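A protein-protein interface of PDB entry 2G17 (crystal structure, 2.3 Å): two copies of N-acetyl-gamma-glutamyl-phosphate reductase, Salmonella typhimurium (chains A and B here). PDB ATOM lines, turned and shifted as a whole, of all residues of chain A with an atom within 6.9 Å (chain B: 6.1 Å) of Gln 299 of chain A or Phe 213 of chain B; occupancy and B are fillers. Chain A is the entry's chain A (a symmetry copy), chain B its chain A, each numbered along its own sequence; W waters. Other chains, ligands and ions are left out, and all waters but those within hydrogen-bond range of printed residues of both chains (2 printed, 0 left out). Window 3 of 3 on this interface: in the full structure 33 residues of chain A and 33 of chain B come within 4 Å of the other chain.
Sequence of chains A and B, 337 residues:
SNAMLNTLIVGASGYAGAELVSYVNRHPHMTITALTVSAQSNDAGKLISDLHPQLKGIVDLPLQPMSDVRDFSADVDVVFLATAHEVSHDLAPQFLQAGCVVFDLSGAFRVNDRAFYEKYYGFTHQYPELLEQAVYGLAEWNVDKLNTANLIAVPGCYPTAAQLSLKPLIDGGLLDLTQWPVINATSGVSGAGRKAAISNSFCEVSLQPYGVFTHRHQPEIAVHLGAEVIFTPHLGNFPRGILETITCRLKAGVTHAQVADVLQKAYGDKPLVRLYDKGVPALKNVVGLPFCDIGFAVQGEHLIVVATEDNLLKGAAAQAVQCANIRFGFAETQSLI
Of the 12 printed residues of chain A, 5 touch a printed residue of chain B. Printed residues of chain B that touch a printed residue of chain A: Trp 180, Val 212, Phe 213, Ile 230 and Thr 232. Hydrophobic or aromatic side chains of chain B within 4 Å of the printed part of chain A: Trp 180, Val 212, Phe 213 and Ile 230. Among the printed residues, no Asp or Glu carboxylate lies within 4 Å of a Lys or Arg side-chain nitrogen of the other chain.
Among the printed residues, pairs that only touch across the chains: Ala 297 of chain A with Val 212 of chain B (3.8 Å), Ala 297 of chain A with Phe 213 of chain B (3.5 Å), Val 298 of chain A with Phe 213 of chain B (3.7 Å), Gln 299 of chain A with Phe 213 of chain B (3.5 Å), His 302 of chain A with Trp 180 of chain B (3.5 Å), His 302 of chain A with Phe 213 of chain B (3.6 Å), His 302 of chain A with Ile 230 of chain B (3.6 Å), Ile 304 of chain A with Val 212 of chain B (3.7 Å), Ile 304 of chain A with Phe 213 of chain B (3.5 Å), Ile 304 of chain A with Ile 230 of chain B (3.9 Å) and Ile 304 of chain A with Thr 232 of chain B (3.4 Å).
O of Ile 304 of chain A is in hydrogen-bond range of N of Ala 297 of chain A, 2.9 Å away.
Gln 299 of chain A touches just one residue of chain B: Phe 213. Phe 213 of chain B touches five residues of chain A. Of the printed residues of chain B, Ile 304 of chain A touches Val 212 (3.7 Å), Phe 213 (3.5 Å), Ile 230 (3.9 Å) and Thr 232 (3.4 Å). Of the printed residues of chain A, Val 212 of chain B touches Ala 297 (3.8 Å) and Ile 304 (3.7 Å). The nearest residue of chain B that does not touch Gln 299 of chain A is Trp 180 of chain B (5.2 Å).
No position is printed for both chains. Of the 11 pairs that touch across the chains among the printed residues, none has its exchanged pair printed and touching as well.
Water W2 bridges the side-chain hydroxyl of Thr 232 of chain B and the side-chain hydroxyl of Thr 247 of chain A. Water W1 bridges NE2 of His 302 of chain A (3.0 Å) and N of Trp 180 of chain B (3.2 Å).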
ATOM      1  N   THR A 247      -2.960  32.609   8.959  1.00  0.00           N
ATOM      2  CA  THR A 247      -3.447  31.248   8.819  1.00  0.00           C
ATOM      3  C   THR A 247      -4.602  31.013   9.782  1.00  0.00           C
ATOM      4  O   THR A 247      -4.467  31.268  10.996  1.00  0.00           O
ATOM      5  CB  THR A 247      -2.297  30.238   9.048  1.00  0.00           C
ATOM      6  OG1 THR A 247      -1.239  30.558   8.130  1.00  0.00           O
ATOM      7  CG2 THR A 247      -2.771  28.776   8.821  1.00  0.00           C
ATOM      8  N   CYS A 248      -5.744  30.581   9.241  1.00  0.00           N
ATOM      9  CA  CYS A 248      -6.937  30.331  10.059  1.00  0.00           C
ATOM     10  C   CYS A 248      -7.611  29.003   9.744  1.00  0.00           C
ATOM     11  O   CYS A 248      -7.393  28.423   8.680  1.00  0.00           O
ATOM     12  CB  CYS A 248      -8.001  31.414   9.841  1.00  0.00           C
ATOM     13  SG  CYS A 248      -7.444  33.086   9.603  1.00  0.00           S
ATOM     14  N   LEU A 250     -11.324  27.620   8.987  1.00  0.00           N
ATOM     15  CA  LEU A 250     -12.679  27.991   8.571  1.00  0.00           C
ATOM     16  C   LEU A 250     -13.708  27.152   9.301  1.00  0.00           C
ATOM     17  O   LEU A 250     -13.422  26.010   9.675  1.00  0.00           O
ATOM     18  CB  LEU A 250     -12.841  27.704   7.073  1.00  0.00           C
ATOM     19  CG  LEU A 250     -12.001  28.542   6.117  1.00  0.00           C
ATOM     20  CD1 LEU A 250     -12.080  27.946   4.732  1.00  0.00           C
ATOM     21  CD2 LEU A 250     -12.522  29.979   6.162  1.00  0.00           C
ATOM     22  N   PHE A 296      -5.673  35.441  -1.081  1.00  0.00           N
ATOM     23  CA  PHE A 296      -5.917  34.344  -0.143  1.00  0.00           C
ATOM     24  C   PHE A 296      -6.008  33.022  -0.883  1.00  0.00           C
ATOM     25  O   PHE A 296      -6.056  33.007  -2.112  1.00  0.00           O
ATOM     26  CB  PHE A 296      -7.179  34.609   0.723  1.00  0.00           C
ATOM     27  CG  PHE A 296      -8.474  34.345   0.004  1.00  0.00           C
ATOM     28  CD1 PHE A 296      -9.096  33.106   0.110  1.00  0.00           C
ATOM     29  CD2 PHE A 296      -9.052  35.319  -0.787  1.00  0.00           C
ATOM     30  CE1 PHE A 296     -10.284  32.825  -0.557  1.00  0.00           C
ATOM     31  CE2 PHE A 296     -10.246  35.058  -1.467  1.00  0.00           C
ATOM     32  CZ  PHE A 296     -10.856  33.814  -1.356  1.00  0.00           C
ATOM     33  N   ALA A 297      -5.965  31.920  -0.133  1.00  0.00           N
ATOM     34  CA  ALA A 297      -6.067  30.572  -0.670  1.00  0.00           C
ATOM     35  C   ALA A 297      -6.756  29.720   0.386  1.00  0.00           C
ATOM     36  O   ALA A 297      -6.658  29.995   1.590  1.00  0.00           O
ATOM     37  CB  ALA A 297      -4.696  30.006  -1.007  1.00  0.00           C
ATOM     38  N   VAL A 298      -7.479  28.711  -0.076  1.00  0.00           N
ATOM     39  CA  VAL A 298      -8.247  27.838   0.801  1.00  0.00           C
ATOM     40  C   VAL A 298      -7.918  26.383   0.460  1.00  0.00           C
ATOM     41  O   VAL A 298      -7.757  26.042  -0.703  1.00  0.00           O
ATOM     42  CB  VAL A 298      -9.760  28.079   0.633  1.00  0.00           C
ATOM     43  CG1 VAL A 298     -10.590  26.883   1.184  1.00  0.00           C
ATOM     44  CG2 VAL A 298     -10.147  29.380   1.289  1.00  0.00           C
ATOM     45  N   GLN A 299      -7.784  25.539   1.468  1.00  0.00           N
ATOM     46  CA  GLN A 299      -7.724  24.115   1.207  1.00  0.00           C
ATOM     47  C   GLN A 299      -8.497  23.423   2.298  1.00  0.00           C
ATOM     48  O   GLN A 299      -8.123  23.493   3.467  1.00  0.00           O
ATOM     49  CB  GLN A 299      -6.286  23.605   1.133  1.00  0.00           C
ATOM     50  CG  GLN A 299      -6.200  22.099   0.784  1.00  0.00           C
ATOM     51  CD  GLN A 299      -4.780  21.592   0.904  1.00  0.00           C
ATOM     52  OE1 GLN A 299      -4.213  21.495   2.009  1.00  0.00           O
ATOM     53  NE2 GLN A 299      -4.177  21.298  -0.239  1.00  0.00           N
ATOM     54  N   GLY A 300      -9.598  22.776   1.920  1.00  0.00           N
ATOM     55  CA  GLY A 300     -10.508  22.206   2.910  1.00  0.00           C
ATOM     56  C   GLY A 300     -10.888  23.262   3.937  1.00  0.00           C
ATOM     57  O   GLY A 300     -11.333  24.345   3.578  1.00  0.00           O
ATOM     58  N   GLU A 301     -10.680  22.962   5.216  1.00  0.00           N
ATOM     59  CA  GLU A 301     -11.056  23.899   6.295  1.00  0.00           C
ATOM     60  C   GLU A 301      -9.957  24.898   6.686  1.00  0.00           C
ATOM     61  O   GLU A 301     -10.113  25.606   7.677  1.00  0.00           O
ATOM     62  CB  GLU A 301     -11.525  23.136   7.552  1.00  0.00           C
ATOM     63  CG  GLU A 301     -10.358  22.517   8.357  1.00  0.00           C
ATOM     64  CD  GLU A 301     -10.780  21.478   9.422  1.00  0.00           C
ATOM     65  OE1 GLU A 301     -11.991  21.447   9.863  1.00  0.00           O
ATOM     66  OE2 GLU A 301      -9.855  20.698   9.813  1.00  0.00           O
ATOM     67  N   HIS A 302      -8.868  24.962   5.912  1.00  0.00           N
ATOM     68  CA  HIS A 302      -7.784  25.900   6.171  1.00  0.00           C
ATOM     69  C   HIS A 302      -7.761  27.065   5.195  1.00  0.00           C
ATOM     70  O   HIS A 302      -7.934  26.908   3.984  1.00  0.00           O
ATOM     71  CB  HIS A 302      -6.431  25.174   6.193  1.00  0.00           C
ATOM     72  CG  HIS A 302      -6.344  24.133   7.274  1.00  0.00           C
ATOM     73  ND1 HIS A 302      -6.491  22.782   7.028  1.00  0.00           N
ATOM     74  CD2 HIS A 302      -6.195  24.258   8.617  1.00  0.00           C
ATOM     75  CE1 HIS A 302      -6.403  22.122   8.167  1.00  0.00           C
ATOM     76  NE2 HIS A 302      -6.218  22.994   9.146  1.00  0.00           N
ATOM     77  N   LEU A 303      -7.541  28.241   5.757  1.00  0.00           N
ATOM     78  CA  LEU A 303      -7.468  29.473   5.017  1.00  0.00           C
ATOM     79  C   LEU A 303      -6.123  30.158   5.316  1.00  0.00           C
ATOM     80  O   LEU A 303      -5.715  30.225   6.487  1.00  0.00           O
ATOM     81  CB  LEU A 303      -8.616  30.396   5.432  1.00  0.00           C
ATOM     82  CG  LEU A 303      -8.497  31.858   4.988  1.00  0.00           C
ATOM     83  CD1 LEU A 303      -8.794  32.019   3.500  1.00  0.00           C
ATOM     84  CD2 LEU A 303      -9.416  32.767   5.810  1.00  0.00           C
ATOM     85  N   ILE A 304      -5.453  30.640   4.256  1.00  0.00           N
ATOM     86  CA  ILE A 304      -4.321  31.537   4.369  1.00  0.00           C
ATOM     87  C   ILE A 304      -4.655  32.860   3.656  1.00  0.00           C
ATOM     88  O   ILE A 304      -4.973  32.866   2.470  1.00  0.00           O
ATOM     89  CB  ILE A 304      -3.036  30.884   3.798  1.00  0.00           C
ATOM     90  CG1 ILE A 304      -2.677  29.608   4.606  1.00  0.00           C
ATOM     91  CG2 ILE A 304      -1.838  31.873   3.753  1.00  0.00           C
ATOM     92  CD1 ILE A 304      -1.658  28.701   3.897  1.00  0.00           C
ATOM     93  N   TRP B 180      -3.302  21.788  13.563  1.00  0.00           N
ATOM     94  CA  TRP B 180      -2.105  21.495  12.746  1.00  0.00           C
ATOM     95  C   TRP B 180      -1.033  22.535  13.010  1.00  0.00           C
ATOM     96  O   TRP B 180      -1.321  23.718  12.988  1.00  0.00           O
ATOM     97  CB  TRP B 180      -2.421  21.517  11.248  1.00  0.00           C
ATOM     98  CG  TRP B 180      -3.389  20.472  10.758  1.00  0.00           C
ATOM     99  CD1 TRP B 180      -4.177  19.641  11.519  1.00  0.00           C
ATOM    100  CD2 TRP B 180      -3.693  20.177   9.394  1.00  0.00           C
ATOM    101  NE1 TRP B 180      -4.953  18.844  10.706  1.00  0.00           N
ATOM    102  CE2 TRP B 180      -4.672  19.143   9.395  1.00  0.00           C
ATOM    103  CE3 TRP B 180      -3.230  20.674   8.166  1.00  0.00           C
ATOM    104  CZ2 TRP B 180      -5.206  18.605   8.201  1.00  0.00           C
ATOM    105  CZ3 TRP B 180      -3.750  20.133   6.973  1.00  0.00           C
ATOM    106  CH2 TRP B 180      -4.731  19.110   7.002  1.00  0.00           C
ATOM    107  N   TYR B 210       4.832  31.513  -1.627  1.00  0.00           N
ATOM    108  CA  TYR B 210       4.635  30.760  -2.871  1.00  0.00           C
ATOM    109  C   TYR B 210       4.324  29.312  -2.509  1.00  0.00           C
ATOM    110  O   TYR B 210       4.432  28.919  -1.337  1.00  0.00           O
ATOM    111  CB  TYR B 210       5.859  30.879  -3.799  1.00  0.00           C
ATOM    112  CG  TYR B 210       7.117  30.233  -3.237  1.00  0.00           C
ATOM    113  CD1 TYR B 210       7.534  28.943  -3.658  1.00  0.00           C
ATOM    114  CD2 TYR B 210       7.895  30.902  -2.297  1.00  0.00           C
ATOM    115  CE1 TYR B 210       8.713  28.347  -3.118  1.00  0.00           C
ATOM    116  CE2 TYR B 210       9.030  30.324  -1.758  1.00  0.00           C
ATOM    117  CZ  TYR B 210       9.444  29.060  -2.176  1.00  0.00           C
ATOM    118  OH  TYR B 210      10.597  28.549  -1.613  1.00  0.00           O
ATOM    119  N   GLY B 211       3.890  28.521  -3.481  1.00  0.00           N
ATOM    120  CA  GLY B 211       3.571  27.115  -3.204  1.00  0.00           C
ATOM    121  C   GLY B 211       2.551  26.996  -2.087  1.00  0.00           C
ATOM    122  O   GLY B 211       2.598  26.050  -1.294  1.00  0.00           O
ATOM    123  N   VAL B 212       1.627  27.958  -2.032  1.00  0.00           N
ATOM    124  CA  VAL B 212       0.618  27.973  -0.988  1.00  0.00           C
ATOM    125  C   VAL B 212      -0.342  26.774  -1.109  1.00  0.00           C
ATOM    126  O   VAL B 212      -1.079  26.645  -2.094  1.00  0.00           O
ATOM    127  CB  VAL B 212      -0.176  29.304  -0.935  1.00  0.00           C
ATOM    128  CG1 VAL B 212      -1.190  29.269   0.222  1.00  0.00           C
ATOM    129  CG2 VAL B 212       0.777  30.461  -0.739  1.00  0.00           C
ATOM    130  N   PHE B 213      -0.321  25.917  -0.089  1.00  0.00           N
ATOM    131  CA  PHE B 213      -1.054  24.647  -0.155  1.00  0.00           C
ATOM    132  C   PHE B 213      -0.617  23.743  -1.328  1.00  0.00           C
ATOM    133  O   PHE B 213      -1.351  22.858  -1.693  1.00  0.00           O
ATOM    134  CB  PHE B 213      -2.583  24.865  -0.242  1.00  0.00           C
ATOM    135  CG  PHE B 213      -3.191  25.466   0.991  1.00  0.00           C
ATOM    136  CD1 PHE B 213      -2.957  24.900   2.249  1.00  0.00           C
ATOM    137  CD2 PHE B 213      -4.031  26.584   0.893  1.00  0.00           C
ATOM    138  CE1 PHE B 213      -3.550  25.454   3.412  1.00  0.00           C
ATOM    139  CE2 PHE B 213      -4.632  27.147   2.035  1.00  0.00           C
ATOM    140  CZ  PHE B 213      -4.388  26.571   3.304  1.00  0.00           C
ATOM    141  N   THR B 214       0.548  23.960  -1.930  1.00  0.00           N
ATOM    142  CA  THR B 214       0.947  23.114  -3.071  1.00  0.00           C
ATOM    143  C   THR B 214       2.412  22.679  -3.040  1.00  0.00           C
ATOM    144  O   THR B 214       2.808  21.828  -3.840  1.00  0.00           O
ATOM    145  CB  THR B 214       0.707  23.785  -4.450  1.00  0.00           C
ATOM    146  OG1 THR B 214       1.502  24.972  -4.545  1.00  0.00           O
ATOM    147  CG2 THR B 214      -0.748  24.122  -4.687  1.00  0.00           C
ATOM    148  N   HIS B 215       3.203  23.231  -2.126  1.00  0.00           N
ATOM    149  CA  HIS B 215       4.627  22.943  -2.106  1.00  0.00           C
ATOM    150  C   HIS B 215       4.941  21.464  -1.784  1.00  0.00           C
ATOM    151  O   HIS B 215       4.388  20.877  -0.852  1.00  0.00           O
ATOM    152  CB  HIS B 215       5.365  23.875  -1.157  1.00  0.00           C
ATOM    153  CG  HIS B 215       6.819  24.020  -1.464  1.00  0.00           C
ATOM    154  ND1 HIS B 215       7.748  23.054  -1.138  1.00  0.00           N
ATOM    155  CD2 HIS B 215       7.514  25.023  -2.053  1.00  0.00           C
ATOM    156  CE1 HIS B 215       8.952  23.454  -1.512  1.00  0.00           C
ATOM    157  NE2 HIS B 215       8.837  24.638  -2.078  1.00  0.00           N
ATOM    158  N   ILE B 230       0.507  22.828   8.395  1.00  0.00           N
ATOM    159  CA  ILE B 230       0.459  23.911   7.407  1.00  0.00           C
ATOM    160  C   ILE B 230       1.914  24.353   7.147  1.00  0.00           C
ATOM    161  O   ILE B 230       2.667  24.617   8.092  1.00  0.00           O
ATOM    162  CB  ILE B 230      -0.405  25.129   7.845  1.00  0.00           C
ATOM    163  CG1 ILE B 230      -1.823  24.692   8.250  1.00  0.00           C
ATOM    164  CG2 ILE B 230      -0.412  26.263   6.725  1.00  0.00           C
ATOM    165  CD1 ILE B 230      -2.701  24.253   7.084  1.00  0.00           C
ATOM    166  N   PHE B 231       2.303  24.389   5.869  1.00  0.00           N
ATOM    167  CA  PHE B 231       3.644  24.799   5.459  1.00  0.00           C
ATOM    168  C   PHE B 231       3.565  25.900   4.395  1.00  0.00           C
ATOM    169  O   PHE B 231       3.057  25.661   3.276  1.00  0.00           O
ATOM    170  CB  PHE B 231       4.482  23.609   4.946  1.00  0.00           C
ATOM    171  CG  PHE B 231       5.808  24.044   4.333  1.00  0.00           C
ATOM    172  CD1 PHE B 231       6.789  24.660   5.126  1.00  0.00           C
ATOM    173  CD2 PHE B 231       6.041  23.907   2.950  1.00  0.00           C
ATOM    174  CE1 PHE B 231       7.978  25.128   4.561  1.00  0.00           C
ATOM    175  CE2 PHE B 231       7.234  24.346   2.373  1.00  0.00           C
ATOM    176  CZ  PHE B 231       8.208  24.940   3.174  1.00  0.00           C
ATOM    177  N   THR B 232       4.014  27.114   4.754  1.00  0.00           N
ATOM    178  CA  THR B 232       4.007  28.229   3.801  1.00  0.00           C
ATOM    179  C   THR B 232       5.393  28.829   3.624  1.00  0.00           C
ATOM    180  O   THR B 232       5.899  29.507   4.520  1.00  0.00           O
ATOM    181  CB  THR B 232       2.957  29.298   4.163  1.00  0.00           C
ATOM    182  OG1 THR B 232       1.702  28.644   4.403  1.00  0.00           O
ATOM    183  CG2 THR B 232       2.777  30.290   3.035  1.00  0.00           C
HETATM  184  O   HOH W   1      -5.949  22.885  12.099  1.00  0.00           O
HETATM  185  O   HOH W   2       1.089  29.630   6.768  1.00  0.00           O
